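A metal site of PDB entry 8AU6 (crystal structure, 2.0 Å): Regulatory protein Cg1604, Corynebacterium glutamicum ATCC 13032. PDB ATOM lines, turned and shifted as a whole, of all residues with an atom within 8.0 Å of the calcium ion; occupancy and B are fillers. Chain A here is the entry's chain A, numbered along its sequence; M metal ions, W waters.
N of Val 241 sits close to OE1 of Glu 291.
ND2 of Asn 268 is in hydrogen-bond range of O of Asp 264 (3.0 Å).
The side-chain carboxylate of Glu 291 lies within hydrogen-bond range of the side-chain hydroxyl of Ser 270 (2.5 Å).
Within 4 Å of the calcium ion: Asp 235, Asn 268 and Glu 291.
The nearest printed residue that does not touch the calcium ion is Gly 240 (4.3 Å).
The calcium ion is bound by the backbone carbonyl oxygen of Asn 268 (2.3 Å), water W2 (2.4 Å), the side-chain carboxylate of Asp 235 (2.4 Å), water W1 (2.4 Å), the side-chain carboxylate of Glu 291 (2.4 Å) and water W3 (2.5 Å).
The calcium ion has six donor atoms within binding distance.
Water W2 bridges the side-chain carboxylate of Asp 235 and the side-chain amide oxygen of Asn 268.
Water W3 lies within hydrogen-bond range of O of Glu 291 and O of Ser 239.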
ATOM      1  N   ALA A 231      -7.189 -18.813 -12.453  1.00  0.00           N
ATOM      2  CA  ALA A 231      -8.562 -18.715 -11.942  1.00  0.00           C
ATOM      3  C   ALA A 231      -9.296 -17.521 -12.546  1.00  0.00           C
ATOM      4  O   ALA A 231     -10.478 -17.636 -12.892  1.00  0.00           O
ATOM      5  CB  ALA A 231      -8.541 -18.608 -10.417  1.00  0.00           C
ATOM      6  N   LEU A 234     -10.338 -18.413 -16.185  1.00  0.00           N
ATOM      7  CA  LEU A 234     -11.519 -19.255 -16.224  1.00  0.00           C
ATOM      8  C   LEU A 234     -12.785 -18.445 -15.977  1.00  0.00           C
ATOM      9  O   LEU A 234     -13.804 -18.629 -16.653  1.00  0.00           O
ATOM     10  CB  LEU A 234     -11.414 -20.365 -15.175  1.00  0.00           C
ATOM     11  CG  LEU A 234     -10.433 -21.516 -15.425  1.00  0.00           C
ATOM     12  CD1 LEU A 234     -10.454 -22.461 -14.234  1.00  0.00           C
ATOM     13  CD2 LEU A 234     -10.790 -22.240 -16.700  1.00  0.00           C
ATOM     14  N   ASP A 235     -12.748 -17.534 -15.001  1.00  0.00           N
ATOM     15  CA  ASP A 235     -13.906 -16.700 -14.712  1.00  0.00           C
ATOM     16  C   ASP A 235     -14.218 -15.746 -15.843  1.00  0.00           C
ATOM     17  O   ASP A 235     -15.387 -15.445 -16.106  1.00  0.00           O
ATOM     18  CB  ASP A 235     -13.674 -15.933 -13.405  1.00  0.00           C
ATOM     19  CG  ASP A 235     -14.909 -15.205 -12.935  1.00  0.00           C
ATOM     20  OD1 ASP A 235     -15.748 -15.831 -12.250  1.00  0.00           O
ATOM     21  OD2 ASP A 235     -15.042 -14.001 -13.242  1.00  0.00           O
ATOM     22  N   ALA A 236     -13.188 -15.254 -16.547  1.00  0.00           N
ATOM     23  CA  ALA A 236     -13.393 -14.326 -17.654  1.00  0.00           C
ATOM     24  C   ALA A 236     -14.101 -14.973 -18.833  1.00  0.00           C
ATOM     25  O   ALA A 236     -14.551 -14.245 -19.733  1.00  0.00           O
ATOM     26  CB  ALA A 236     -12.051 -13.753 -18.111  1.00  0.00           C
ATOM     27  N   GLY A 238     -16.948 -16.369 -18.599  1.00  0.00           N
ATOM     28  CA  GLY A 238     -18.301 -16.520 -18.111  1.00  0.00           C
ATOM     29  C   GLY A 238     -18.381 -17.586 -17.028  1.00  0.00           C
ATOM     30  O   GLY A 238     -17.407 -17.911 -16.343  1.00  0.00           O
ATOM     31  N   SER A 239     -19.601 -18.124 -16.870  1.00  0.00           N
ATOM     32  CA  SER A 239     -19.863 -19.238 -15.971  1.00  0.00           C
ATOM     33  C   SER A 239     -19.631 -18.869 -14.515  1.00  0.00           C
ATOM     34  O   SER A 239     -20.453 -18.163 -13.906  1.00  0.00           O
ATOM     35  CB  SER A 239     -19.004 -20.445 -16.380  1.00  0.00           C
ATOM     36  OG  SER A 239     -19.129 -20.709 -17.767  1.00  0.00           O
ATOM     37  N   GLY A 240     -18.534 -19.340 -13.920  1.00  0.00           N
ATOM     38  CA  GLY A 240     -18.242 -19.052 -12.530  1.00  0.00           C
ATOM     39  C   GLY A 240     -17.157 -19.924 -11.939  1.00  0.00           C
ATOM     40  O   GLY A 240     -17.012 -21.084 -12.329  1.00  0.00           O
ATOM     41  N   VAL A 241     -16.360 -19.388 -11.007  1.00  0.00           N
ATOM     42  CA  VAL A 241     -15.218 -20.103 -10.446  1.00  0.00           C
ATOM     43  C   VAL A 241     -15.211 -19.932  -8.930  1.00  0.00           C
ATOM     44  O   VAL A 241     -15.414 -18.824  -8.406  1.00  0.00           O
ATOM     45  CB  VAL A 241     -13.881 -19.602 -11.048  1.00  0.00           C
ATOM     46  CG1 VAL A 241     -12.722 -20.405 -10.478  1.00  0.00           C
ATOM     47  CG2 VAL A 241     -13.907 -19.705 -12.565  1.00  0.00           C
ATOM     48  N   VAL A 242     -14.962 -21.031  -8.230  1.00  0.00           N
ATOM     49  CA  VAL A 242     -14.762 -21.034  -6.777  1.00  0.00           C
ATOM     50  C   VAL A 242     -13.399 -21.647  -6.496  1.00  0.00           C
ATOM     51  O   VAL A 242     -13.139 -22.795  -6.886  1.00  0.00           O
ATOM     52  CB  VAL A 242     -15.860 -21.801  -6.039  1.00  0.00           C
ATOM     53  CG1 VAL A 242     -15.634 -21.735  -4.537  1.00  0.00           C
ATOM     54  CG2 VAL A 242     -17.239 -21.259  -6.398  1.00  0.00           C
ATOM     55  N   ASP A 264     -10.821  -6.606  -8.979  1.00  0.00           N
ATOM     56  CA  ASP A 264     -11.644  -7.277  -9.982  1.00  0.00           C
ATOM     57  C   ASP A 264     -11.814  -8.754  -9.679  1.00  0.00           C
ATOM     58  O   ASP A 264     -12.912  -9.311  -9.822  1.00  0.00           O
ATOM     59  CB  ASP A 264     -11.045  -7.076 -11.369  1.00  0.00           C
ATOM     60  CG  ASP A 264     -10.768  -5.625 -11.686  1.00  0.00           C
ATOM     61  OD1 ASP A 264     -11.525  -4.751 -11.192  1.00  0.00           O
ATOM     62  OD2 ASP A 264      -9.799  -5.347 -12.424  1.00  0.00           O
ATOM     63  N   ALA A 265     -10.733  -9.410  -9.239  1.00  0.00           N
ATOM     64  CA  ALA A 265     -10.806 -10.840  -8.947  1.00  0.00           C
ATOM     65  C   ALA A 265     -11.598 -11.107  -7.670  1.00  0.00           C
ATOM     66  O   ALA A 265     -12.367 -12.070  -7.604  1.00  0.00           O
ATOM     67  CB  ALA A 265      -9.402 -11.431  -8.836  1.00  0.00           C
ATOM     68  N   GLU A 267     -14.101  -9.585  -6.530  1.00  0.00           N
ATOM     69  CA  GLU A 267     -15.529  -9.489  -6.798  1.00  0.00           C
ATOM     70  C   GLU A 267     -16.030 -10.632  -7.668  1.00  0.00           C
ATOM     71  O   GLU A 267     -17.196 -11.038  -7.557  1.00  0.00           O
ATOM     72  CB  GLU A 267     -15.843  -8.147  -7.474  1.00  0.00           C
ATOM     73  CG  GLU A 267     -17.306  -7.939  -7.821  1.00  0.00           C
ATOM     74  CD  GLU A 267     -17.507  -6.855  -8.867  1.00  0.00           C
ATOM     75  OE1 GLU A 267     -16.519  -6.181  -9.227  1.00  0.00           O
ATOM     76  OE2 GLU A 267     -18.653  -6.695  -9.340  1.00  0.00           O
ATOM     77  N   ASN A 268     -15.167 -11.174  -8.540  1.00  0.00           N
ATOM     78  CA  ASN A 268     -15.598 -12.153  -9.534  1.00  0.00           C
ATOM     79  C   ASN A 268     -15.328 -13.594  -9.137  1.00  0.00           C
ATOM     80  O   ASN A 268     -16.080 -14.480  -9.546  1.00  0.00           O
ATOM     81  CB  ASN A 268     -14.898 -11.864 -10.874  1.00  0.00           C
ATOM     82  CG  ASN A 268     -15.337 -10.550 -11.489  1.00  0.00           C
ATOM     83  OD1 ASN A 268     -16.440 -10.071 -11.234  1.00  0.00           O
ATOM     84  ND2 ASN A 268     -14.474  -9.967 -12.314  1.00  0.00           N
ATOM     85  N   VAL A 269     -14.283 -13.865  -8.359  1.00  0.00           N
ATOM     86  CA  VAL A 269     -13.892 -15.239  -8.016  1.00  0.00           C
ATOM     87  C   VAL A 269     -14.103 -15.445  -6.524  1.00  0.00           C
ATOM     88  O   VAL A 269     -13.504 -14.736  -5.703  1.00  0.00           O
ATOM     89  CB  VAL A 269     -12.436 -15.521  -8.417  1.00  0.00           C
ATOM     90  CG1 VAL A 269     -12.038 -16.916  -7.976  1.00  0.00           C
ATOM     91  CG2 VAL A 269     -12.259 -15.357  -9.912  1.00  0.00           C
ATOM     92  N   SER A 270     -14.926 -16.425  -6.177  1.00  0.00           N
ATOM     93  CA  SER A 270     -15.125 -16.776  -4.778  1.00  0.00           C
ATOM     94  C   SER A 270     -13.895 -17.487  -4.229  1.00  0.00           C
ATOM     95  O   SER A 270     -13.290 -18.325  -4.898  1.00  0.00           O
ATOM     96  CB  SER A 270     -16.359 -17.675  -4.617  1.00  0.00           C
ATOM     97  OG  SER A 270     -17.526 -17.019  -5.058  1.00  0.00           O
ATOM     98  N   SER A 287     -20.912 -21.185  -2.276  1.00  0.00           N
ATOM     99  CA  SER A 287     -20.305 -20.270  -3.237  1.00  0.00           C
ATOM    100  C   SER A 287     -20.601 -20.681  -4.677  1.00  0.00           C
ATOM    101  O   SER A 287     -20.676 -19.817  -5.560  1.00  0.00           O
ATOM    102  CB  SER A 287     -18.786 -20.200  -3.008  1.00  0.00           C
ATOM    103  OG  SER A 287     -18.488 -19.670  -1.738  1.00  0.00           O
ATOM    104  N   GLU A 290     -23.724 -19.111  -5.460  1.00  0.00           N
ATOM    105  CA  GLU A 290     -23.498 -17.674  -5.629  1.00  0.00           C
ATOM    106  C   GLU A 290     -22.925 -17.362  -7.003  1.00  0.00           C
ATOM    107  O   GLU A 290     -23.358 -16.417  -7.662  1.00  0.00           O
ATOM    108  CB  GLU A 290     -22.555 -17.153  -4.544  1.00  0.00           C
ATOM    109  CG  GLU A 290     -23.050 -17.340  -3.127  1.00  0.00           C
ATOM    110  CD  GLU A 290     -22.139 -16.682  -2.104  1.00  0.00           C
ATOM    111  OE1 GLU A 290     -21.756 -15.518  -2.328  1.00  0.00           O
ATOM    112  OE2 GLU A 290     -21.794 -17.336  -1.099  1.00  0.00           O
ATOM    113  N   GLU A 291     -21.944 -18.147  -7.451  1.00  0.00           N
ATOM    114  CA  GLU A 291     -21.347 -17.923  -8.763  1.00  0.00           C
ATOM    115  C   GLU A 291     -22.359 -18.127  -9.881  1.00  0.00           C
ATOM    116  O   GLU A 291     -22.277 -17.449 -10.917  1.00  0.00           O
ATOM    117  CB  GLU A 291     -20.146 -18.846  -8.966  1.00  0.00           C
ATOM    118  CG  GLU A 291     -18.967 -18.523  -8.068  1.00  0.00           C
ATOM    119  CD  GLU A 291     -18.373 -17.164  -8.384  1.00  0.00           C
ATOM    120  OE1 GLU A 291     -18.146 -16.866  -9.573  1.00  0.00           O
ATOM    121  OE2 GLU A 291     -18.133 -16.384  -7.432  1.00  0.00           O
ATOM    122  N   LEU A 292     -23.322 -19.026  -9.685  1.00  0.00           N
ATOM    123  CA  LEU A 292     -24.356 -19.248 -10.699  1.00  0.00           C
ATOM    124  C   LEU A 292     -25.273 -18.047 -10.823  1.00  0.00           C
ATOM    125  O   LEU A 292     -25.716 -17.706 -11.929  1.00  0.00           O
ATOM    126  CB  LEU A 292     -25.145 -20.503 -10.367  1.00  0.00           C
ATOM    127  CG  LEU A 292     -24.452 -21.836 -10.626  1.00  0.00           C
ATOM    128  CD1 LEU A 292     -25.158 -22.959  -9.895  1.00  0.00           C
ATOM    129  CD2 LEU A 292     -24.404 -22.127 -12.110  1.00  0.00           C
ATOM    130  N   ALA A 293     -25.588 -17.387  -9.705  1.00  0.00           N
ATOM    131  CA  ALA A 293     -26.509 -16.254  -9.718  1.00  0.00           C
ATOM    132  C   ALA A 293     -25.869 -15.030 -10.368  1.00  0.00           C
ATOM    133  O   ALA A 293     -24.650 -14.935 -10.483  1.00  0.00           O
ATOM    134  CB  ALA A 293     -26.948 -15.918  -8.296  1.00  0.00           C
HETATM  135 CA    CA M   1     -17.649 -15.053 -11.072  1.00  0.00          CA
HETATM  136  O   HOH W   1     -19.013 -13.624  -9.759  1.00  0.00           O
HETATM  137  O   HOH W   2     -17.845 -13.038 -12.271  1.00  0.00           O
HETATM  138  O   HOH W   3     -19.780 -16.167 -11.675  1.00  0.00           O
